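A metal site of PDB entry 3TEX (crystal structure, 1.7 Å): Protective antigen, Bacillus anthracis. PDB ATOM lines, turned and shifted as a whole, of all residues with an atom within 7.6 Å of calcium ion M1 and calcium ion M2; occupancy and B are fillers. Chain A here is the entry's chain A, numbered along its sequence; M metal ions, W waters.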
ATOM      1  N   TYR A  22     -12.178  25.464 -27.299  1.00  0.00           N
ATOM      2  CA  TYR A  22     -13.293  25.225 -28.196  1.00  0.00           C
ATOM      3  C   TYR A  22     -13.929  26.568 -28.527  1.00  0.00           C
ATOM      4  O   TYR A  22     -14.393  27.272 -27.635  1.00  0.00           O
ATOM      5  CB  TYR A  22     -14.325  24.332 -27.525  1.00  0.00           C
ATOM      6  CG  TYR A  22     -13.786  22.985 -27.145  1.00  0.00           C
ATOM      7  CD1 TYR A  22     -13.346  22.733 -25.860  1.00  0.00           C
ATOM      8  CD2 TYR A  22     -13.688  21.966 -28.081  1.00  0.00           C
ATOM      9  CE1 TYR A  22     -12.831  21.487 -25.513  1.00  0.00           C
ATOM     10  CE2 TYR A  22     -13.182  20.734 -27.751  1.00  0.00           C
ATOM     11  CZ  TYR A  22     -12.757  20.501 -26.471  1.00  0.00           C
ATOM     12  OH  TYR A  22     -12.255  19.269 -26.150  1.00  0.00           O
ATOM     13  N   PRO A 176     -20.070  18.392 -25.121  1.00  0.00           N
ATOM     14  CA  PRO A 176     -20.276  16.948 -25.234  1.00  0.00           C
ATOM     15  C   PRO A 176     -19.039  16.272 -25.828  1.00  0.00           C
ATOM     16  O   PRO A 176     -18.658  16.577 -26.951  1.00  0.00           O
ATOM     17  CB  PRO A 176     -21.469  16.829 -26.175  1.00  0.00           C
ATOM     18  CG  PRO A 176     -22.174  18.172 -26.081  1.00  0.00           C
ATOM     19  CD  PRO A 176     -21.071  19.161 -25.887  1.00  0.00           C
ATOM     20  N   ASP A 177     -18.426  15.389 -25.051  1.00  0.00           N
ATOM     21  CA  ASP A 177     -17.240  14.654 -25.453  1.00  0.00           C
ATOM     22  C   ASP A 177     -17.312  13.346 -24.672  1.00  0.00           C
ATOM     23  O   ASP A 177     -16.553  13.145 -23.716  1.00  0.00           O
ATOM     24  CB  ASP A 177     -15.999  15.450 -25.069  1.00  0.00           C
ATOM     25  CG  ASP A 177     -14.719  14.765 -25.476  1.00  0.00           C
ATOM     26  OD1 ASP A 177     -14.804  13.915 -26.391  1.00  0.00           O
ATOM     27  OD2 ASP A 177     -13.647  15.072 -24.926  1.00  0.00           O
ATOM     28  N   ARG A 178     -18.258  12.496 -25.054  1.00  0.00           N
ATOM     29  CA  ARG A 178     -18.618  11.289 -24.308  1.00  0.00           C
ATOM     30  C   ARG A 178     -17.424  10.350 -24.040  1.00  0.00           C
ATOM     31  O   ARG A 178     -17.368   9.705 -22.997  1.00  0.00           O
ATOM     32  CB  ARG A 178     -19.756  10.544 -25.054  1.00  0.00           C
ATOM     33  CG  ARG A 178     -21.060  11.369 -25.217  1.00  0.00           C
ATOM     34  CD  ARG A 178     -21.995  10.833 -26.308  1.00  0.00           C
ATOM     35  NE  ARG A 178     -22.873   9.747 -25.850  1.00  0.00           N
ATOM     36  CZ  ARG A 178     -23.874   9.918 -25.003  1.00  0.00           C
ATOM     37  NH1 ARG A 178     -24.116  11.124 -24.513  1.00  0.00           N
ATOM     38  NH2 ARG A 178     -24.624   8.890 -24.638  1.00  0.00           N
ATOM     39  N   ASP A 179     -16.467  10.294 -24.965  1.00  0.00           N
ATOM     40  CA  ASP A 179     -15.318   9.392 -24.808  1.00  0.00           C
ATOM     41  C   ASP A 179     -14.041  10.072 -24.268  1.00  0.00           C
ATOM     42  O   ASP A 179     -12.994   9.449 -24.130  1.00  0.00           O
ATOM     43  CB  ASP A 179     -15.024   8.673 -26.127  1.00  0.00           C
ATOM     44  CG  ASP A 179     -14.758   9.629 -27.260  1.00  0.00           C
ATOM     45  OD1 ASP A 179     -14.558  10.838 -26.997  1.00  0.00           O
ATOM     46  OD2 ASP A 179     -14.743   9.175 -28.422  1.00  0.00           O
ATOM     47  N   ASN A 180     -14.128  11.361 -23.967  1.00  0.00           N
ATOM     48  CA  ASN A 180     -12.997  12.098 -23.443  1.00  0.00           C
ATOM     49  C   ASN A 180     -11.738  12.101 -24.315  1.00  0.00           C
ATOM     50  O   ASN A 180     -10.620  12.175 -23.797  1.00  0.00           O
ATOM     51  CB  ASN A 180     -12.600  11.600 -22.049  1.00  0.00           C
ATOM     52  CG  ASN A 180     -11.913  12.683 -21.217  1.00  0.00           C
ATOM     53  OD1 ASN A 180     -12.320  13.840 -21.243  1.00  0.00           O
ATOM     54  ND2 ASN A 180     -10.863  12.308 -20.508  1.00  0.00           N
ATOM     55  N   ASP A 181     -11.876  12.030 -25.637  1.00  0.00           N
ATOM     56  CA  ASP A 181     -10.659  12.169 -26.425  1.00  0.00           C
ATOM     57  C   ASP A 181     -10.326  13.616 -26.727  1.00  0.00           C
ATOM     58  O   ASP A 181      -9.221  13.915 -27.179  1.00  0.00           O
ATOM     59  CB  ASP A 181     -10.651  11.295 -27.699  1.00  0.00           C
ATOM     60  CG  ASP A 181     -11.810  11.581 -28.625  1.00  0.00           C
ATOM     61  OD1 ASP A 181     -12.421  12.682 -28.594  1.00  0.00           O
ATOM     62  OD2 ASP A 181     -12.121  10.686 -29.430  1.00  0.00           O
ATOM     63  N   GLY A 182     -11.265  14.520 -26.462  1.00  0.00           N
ATOM     64  CA  GLY A 182     -11.079  15.925 -26.804  1.00  0.00           C
ATOM     65  C   GLY A 182     -11.869  16.434 -28.000  1.00  0.00           C
ATOM     66  O   GLY A 182     -12.114  17.635 -28.101  1.00  0.00           O
ATOM     67  N   ILE A 183     -12.282  15.542 -28.905  1.00  0.00           N
ATOM     68  CA  ILE A 183     -13.061  15.970 -30.064  1.00  0.00           C
ATOM     69  C   ILE A 183     -14.546  15.926 -29.718  1.00  0.00           C
ATOM     70  O   ILE A 183     -15.055  14.897 -29.318  1.00  0.00           O
ATOM     71  CB  ILE A 183     -12.814  15.054 -31.272  1.00  0.00           C
ATOM     72  CG1 ILE A 183     -11.308  14.882 -31.523  1.00  0.00           C
ATOM     73  CG2 ILE A 183     -13.507  15.625 -32.516  1.00  0.00           C
ATOM     74  CD1 ILE A 183     -10.961  13.852 -32.610  1.00  0.00           C
ATOM     75  N   PRO A 184     -15.245  17.067 -29.844  1.00  0.00           N
ATOM     76  CA  PRO A 184     -16.674  17.113 -29.539  1.00  0.00           C
ATOM     77  C   PRO A 184     -17.470  16.050 -30.296  1.00  0.00           C
ATOM     78  O   PRO A 184     -17.172  15.782 -31.470  1.00  0.00           O
ATOM     79  CB  PRO A 184     -17.077  18.513 -30.015  1.00  0.00           C
ATOM     80  CG  PRO A 184     -15.834  19.334 -29.792  1.00  0.00           C
ATOM     81  CD  PRO A 184     -14.696  18.396 -30.168  1.00  0.00           C
ATOM     82  N   ASP A 185     -18.463  15.449 -29.635  1.00  0.00           N
ATOM     83  CA  ASP A 185     -19.357  14.460 -30.255  1.00  0.00           C
ATOM     84  C   ASP A 185     -19.746  14.840 -31.687  1.00  0.00           C
ATOM     85  O   ASP A 185     -19.612  14.047 -32.623  1.00  0.00           O
ATOM     86  CB  ASP A 185     -20.674  14.352 -29.481  1.00  0.00           C
ATOM     87  CG  ASP A 185     -20.513  13.781 -28.081  1.00  0.00           C
ATOM     88  OD1 ASP A 185     -19.385  13.507 -27.626  1.00  0.00           O
ATOM     89  OD2 ASP A 185     -21.562  13.639 -27.402  1.00  0.00           O
ATOM     90  N   SER A 186     -20.287  16.047 -31.843  1.00  0.00           N
ATOM     91  CA  SER A 186     -20.866  16.456 -33.102  1.00  0.00           C
ATOM     92  C   SER A 186     -19.861  16.454 -34.250  1.00  0.00           C
ATOM     93  O   SER A 186     -20.222  16.141 -35.381  1.00  0.00           O
ATOM     94  CB  SER A 186     -21.527  17.841 -32.971  1.00  0.00           C
ATOM     95  OG  SER A 186     -20.602  18.810 -32.525  1.00  0.00           O
ATOM     96  N   GLU A 188     -17.086  14.510 -34.468  1.00  0.00           N
ATOM     97  CA  GLU A 188     -16.716  13.124 -34.786  1.00  0.00           C
ATOM     98  C   GLU A 188     -17.778  12.473 -35.657  1.00  0.00           C
ATOM     99  O   GLU A 188     -17.459  11.727 -36.589  1.00  0.00           O
ATOM    100  CB  GLU A 188     -16.522  12.310 -33.499  1.00  0.00           C
ATOM    101  CG  GLU A 188     -15.344  12.757 -32.666  1.00  0.00           C
ATOM    102  CD  GLU A 188     -14.829  11.651 -31.768  1.00  0.00           C
ATOM    103  OE1 GLU A 188     -14.223  10.695 -32.300  1.00  0.00           O
ATOM    104  OE2 GLU A 188     -15.035  11.738 -30.536  1.00  0.00           O
ATOM    105  N   TYR A 192     -14.855  16.096 -39.738  1.00  0.00           N
ATOM    106  CA  TYR A 192     -13.968  17.197 -39.382  1.00  0.00           C
ATOM    107  C   TYR A 192     -12.693  17.133 -40.196  1.00  0.00           C
ATOM    108  O   TYR A 192     -12.364  16.109 -40.804  1.00  0.00           O
ATOM    109  CB  TYR A 192     -13.622  17.159 -37.896  1.00  0.00           C
ATOM    110  CG  TYR A 192     -13.067  15.845 -37.372  1.00  0.00           C
ATOM    111  CD1 TYR A 192     -13.911  14.770 -37.099  1.00  0.00           C
ATOM    112  CD2 TYR A 192     -11.717  15.715 -37.077  1.00  0.00           C
ATOM    113  CE1 TYR A 192     -13.398  13.572 -36.589  1.00  0.00           C
ATOM    114  CE2 TYR A 192     -11.188  14.520 -36.562  1.00  0.00           C
ATOM    115  CZ  TYR A 192     -12.051  13.464 -36.304  1.00  0.00           C
ATOM    116  OH  TYR A 192     -11.553  12.285 -35.798  1.00  0.00           O
ATOM    117  N   SER A 221     -15.157   9.738 -36.870  1.00  0.00           N
ATOM    118  CA  SER A 221     -14.772   8.767 -35.854  1.00  0.00           C
ATOM    119  C   SER A 221     -15.916   8.531 -34.881  1.00  0.00           C
ATOM    120  O   SER A 221     -16.907   9.237 -34.921  1.00  0.00           O
ATOM    121  CB  SER A 221     -13.510   9.241 -35.107  1.00  0.00           C
ATOM    122  OG  SER A 221     -13.551  10.646 -34.854  1.00  0.00           O
ATOM    123  N   SER A 222     -15.809   7.523 -34.026  1.00  0.00           N
ATOM    124  CA  SER A 222     -16.883   7.294 -33.048  1.00  0.00           C
ATOM    125  C   SER A 222     -16.780   8.260 -31.870  1.00  0.00           C
ATOM    126  O   SER A 222     -15.755   8.352 -31.240  1.00  0.00           O
ATOM    127  CB  SER A 222     -16.851   5.879 -32.491  1.00  0.00           C
ATOM    128  OG  SER A 222     -17.759   5.826 -31.393  1.00  0.00           O
ATOM    129  N   PRO A 223     -17.885   8.933 -31.543  1.00  0.00           N
ATOM    130  CA  PRO A 223     -17.911   9.828 -30.380  1.00  0.00           C
ATOM    131  C   PRO A 223     -17.899   9.057 -29.053  1.00  0.00           C
ATOM    132  O   PRO A 223     -17.792   9.648 -27.968  1.00  0.00           O
ATOM    133  CB  PRO A 223     -19.232  10.578 -30.558  1.00  0.00           C
ATOM    134  CG  PRO A 223     -20.118   9.592 -31.256  1.00  0.00           C
ATOM    135  CD  PRO A 223     -19.182   8.889 -32.237  1.00  0.00           C
ATOM    136  N   GLU A 224     -17.990   7.730 -29.134  1.00  0.00           N
ATOM    137  CA  GLU A 224     -18.031   6.903 -27.938  1.00  0.00           C
ATOM    138  C   GLU A 224     -16.832   5.948 -27.790  1.00  0.00           C
ATOM    139  O   GLU A 224     -16.721   5.198 -26.814  1.00  0.00           O
ATOM    140  CB  GLU A 224     -19.369   6.159 -27.896  1.00  0.00           C
ATOM    141  CG  GLU A 224     -20.525   7.165 -27.802  1.00  0.00           C
ATOM    142  CD  GLU A 224     -21.890   6.537 -27.673  1.00  0.00           C
ATOM    143  OE1 GLU A 224     -21.956   5.327 -27.354  1.00  0.00           O
ATOM    144  OE2 GLU A 224     -22.897   7.254 -27.867  1.00  0.00           O
ATOM    145  N   LYS A 225     -15.913   6.011 -28.753  1.00  0.00           N
ATOM    146  CA  LYS A 225     -14.667   5.303 -28.641  1.00  0.00           C
ATOM    147  C   LYS A 225     -13.492   6.273 -28.615  1.00  0.00           C
ATOM    148  O   LYS A 225     -13.281   7.032 -29.557  1.00  0.00           O
ATOM    149  CB  LYS A 225     -14.504   4.328 -29.806  1.00  0.00           C
ATOM    150  CG  LYS A 225     -15.595   3.268 -29.855  1.00  0.00           C
ATOM    151  CD  LYS A 225     -15.410   2.371 -31.092  1.00  0.00           C
ATOM    152  CE  LYS A 225     -14.123   1.564 -30.998  1.00  0.00           C
ATOM    153  NZ  LYS A 225     -14.215   0.451 -30.022  1.00  0.00           N
ATOM    154  N   TRP A 226     -12.741   6.246 -27.525  1.00  0.00           N
ATOM    155  CA  TRP A 226     -11.580   7.105 -27.345  1.00  0.00           C
ATOM    156  C   TRP A 226     -10.580   6.861 -28.483  1.00  0.00           C
ATOM    157  O   TRP A 226     -10.041   7.799 -29.068  1.00  0.00           O
ATOM    158  CB  TRP A 226     -10.976   6.799 -25.975  1.00  0.00           C
ATOM    159  CG  TRP A 226      -9.744   7.543 -25.588  1.00  0.00           C
ATOM    160  CD1 TRP A 226      -9.684   8.784 -25.002  1.00  0.00           C
ATOM    161  CD2 TRP A 226      -8.399   7.091 -25.716  1.00  0.00           C
ATOM    162  NE1 TRP A 226      -8.377   9.131 -24.780  1.00  0.00           N
ATOM    163  CE2 TRP A 226      -7.565   8.105 -25.190  1.00  0.00           C
ATOM    164  CE3 TRP A 226      -7.813   5.916 -26.223  1.00  0.00           C
ATOM    165  CZ2 TRP A 226      -6.169   7.983 -25.172  1.00  0.00           C
ATOM    166  CZ3 TRP A 226      -6.422   5.799 -26.191  1.00  0.00           C
ATOM    167  CH2 TRP A 226      -5.614   6.830 -25.666  1.00  0.00           C
ATOM    168  N   SER A 227     -10.332   5.585 -28.783  1.00  0.00           N
ATOM    169  CA  SER A 227      -9.673   5.199 -30.027  1.00  0.00           C
ATOM    170  C   SER A 227     -10.665   4.421 -30.863  1.00  0.00           C
ATOM    171  O   SER A 227     -11.107   3.327 -30.470  1.00  0.00           O
ATOM    172  CB  SER A 227      -8.452   4.324 -29.768  1.00  0.00           C
ATOM    173  OG  SER A 227      -7.874   3.896 -30.991  1.00  0.00           O
ATOM    174  N   THR A 228     -11.033   4.966 -32.010  1.00  0.00           N
ATOM    175  CA  THR A 228     -12.074   4.350 -32.825  1.00  0.00           C
ATOM    176  C   THR A 228     -11.605   3.013 -33.417  1.00  0.00           C
ATOM    177  O   THR A 228     -12.403   2.119 -33.611  1.00  0.00           O
ATOM    178  CB  THR A 228     -12.592   5.327 -33.895  1.00  0.00           C
ATOM    179  OG1 THR A 228     -13.316   6.382 -33.218  1.00  0.00           O
ATOM    180  CG2 THR A 228     -13.552   4.634 -34.851  1.00  0.00           C
ATOM    181  N   SER A 234      -5.429   7.853 -29.086  1.00  0.00           N
ATOM    182  CA  SER A 234      -6.756   8.430 -29.211  1.00  0.00           C
ATOM    183  C   SER A 234      -7.012   9.113 -30.562  1.00  0.00           C
ATOM    184  O   SER A 234      -6.073   9.489 -31.269  1.00  0.00           O
ATOM    185  CB  SER A 234      -7.050   9.424 -28.092  1.00  0.00           C
ATOM    186  OG  SER A 234      -6.817  10.752 -28.506  1.00  0.00           O
ATOM    187  N   ASP A 235      -8.290   9.291 -30.884  1.00  0.00           N
ATOM    188  CA  ASP A 235      -8.663   9.892 -32.168  1.00  0.00           C
ATOM    189  C   ASP A 235      -8.047  11.295 -32.291  1.00  0.00           C
ATOM    190  O   ASP A 235      -7.542  11.698 -33.333  1.00  0.00           O
ATOM    191  CB  ASP A 235     -10.187   9.938 -32.287  1.00  0.00           C
ATOM    192  CG  ASP A 235     -10.829   8.561 -32.336  1.00  0.00           C
ATOM    193  OD1 ASP A 235     -10.162   7.574 -32.731  1.00  0.00           O
ATOM    194  OD2 ASP A 235     -12.036   8.479 -32.023  1.00  0.00           O
ATOM    195  N   PHE A 236      -8.045  12.012 -31.174  1.00  0.00           N
ATOM    196  CA  PHE A 236      -7.474  13.342 -31.099  1.00  0.00           C
ATOM    197  C   PHE A 236      -5.949  13.342 -31.150  1.00  0.00           C
ATOM    198  O   PHE A 236      -5.348  14.188 -31.836  1.00  0.00           O
ATOM    199  CB  PHE A 236      -7.969  13.998 -29.798  1.00  0.00           C
ATOM    200  CG  PHE A 236      -7.480  15.405 -29.581  1.00  0.00           C
ATOM    201  CD1 PHE A 236      -8.041  16.465 -30.268  1.00  0.00           C
ATOM    202  CD2 PHE A 236      -6.529  15.673 -28.608  1.00  0.00           C
ATOM    203  CE1 PHE A 236      -7.623  17.775 -30.037  1.00  0.00           C
ATOM    204  CE2 PHE A 236      -6.091  16.986 -28.362  1.00  0.00           C
ATOM    205  CZ  PHE A 236      -6.655  18.041 -29.081  1.00  0.00           C
ATOM    206  N   PRO A 254      -8.006   8.176 -37.697  1.00  0.00           N
ATOM    207  CA  PRO A 254      -8.716   7.477 -36.612  1.00  0.00           C
ATOM    208  C   PRO A 254      -9.365   6.157 -37.022  1.00  0.00           C
ATOM    209  O   PRO A 254      -9.688   5.372 -36.122  1.00  0.00           O
ATOM    210  CB  PRO A 254      -9.783   8.504 -36.176  1.00  0.00           C
ATOM    211  CG  PRO A 254      -9.155   9.818 -36.467  1.00  0.00           C
ATOM    212  CD  PRO A 254      -8.412   9.602 -37.784  1.00  0.00           C
HETATM  213 CA    CA M   1     -14.864  12.755 -28.427  1.00  0.00          CA
HETATM  214 CA    CA M   2     -13.665   9.208 -30.480  1.00  0.00          CA
HETATM  215  O   HOH W   1     -17.261  12.155 -28.267  1.00  0.00           O
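Five residues have an atom within 4 Å of calcium ion M1: Asp 177, Asp 179, Asp 181, Ile 183 and Glu 188.
Calcium ion M1 is bound by the backbone carbonyl oxygen (O) of Ile 183 (2.3 Å), the side-chain carboxylate (OD1) of Asp 177 (2.3 Å), the side-chain carboxylate (OE2) of Glu 188 (2.3 Å), the side-chain carboxylate (OD1) of Asp 179 (2.4 Å), the side-chain carboxylate (OD1) of Asp 181 (2.4 Å) and water W1 (2.5 Å).
Calcium ion M1 has six donor atoms within binding distance.
Thr 228 touches calcium ion M2.
Of the 26 residues printed, 7 come within 4 Å of calcium ion M2.
The nearest printed residue that does not touch calcium ion M2 is Trp 226 (4.1 Å).
Water W1 lies within hydrogen-bond range of the backbone carbonyl oxygen of Pro 223 (2.6 Å), the side-chain carboxylate of Asp 185 (2.6 Å) and the backbone NH of Arg 178 (3.4 Å).
Calcium ion M2 is bound by OD2 of Asp 179 (2.3 Å), OD2 of Asp 235 (2.4 Å), OD2 of Asp 181 (2.4 Å), O of Ser 222 (2.4 Å), O of Lys 225 (2.4 Å), OE1 of Glu 188 (2.4 Å) and OE2 of Glu 188 (2.9 Å).
The backbone NH of Asp 179 lies close to the backbone carbonyl oxygen of Pro 223 (3.3 Å).
The side-chain hydroxyl (OG) of Ser 222 is in hydrogen-bond range of the backbone NH (N) of Lys 225.
The backbone NH of Gly 182 sits at hydrogen-bond distance from the side-chain carboxylate of Asp 177.
The backbone NH of Ser 221 sits at hydrogen-bond distance from the backbone carbonyl oxygen of Glu 188, at 3.1 Å.
The side-chain carboxylate (OD1) of Asp 235 lies within hydrogen-bond range of the backbone NH (N) of Thr 228, 2.8 Å away.
The backbone NH of Glu 224 sits at hydrogen-bond distance from the side-chain hydroxyl of Ser 222, 3.0 Å away.
N of Ser 222 sits at hydrogen-bond distance from OG1 of Thr 228 (2.9 Å).
The backbone NH (N) of Asp 235 sits at hydrogen-bond distance from the backbone carbonyl oxygen (O) of Trp 226, at 2.9 Å.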
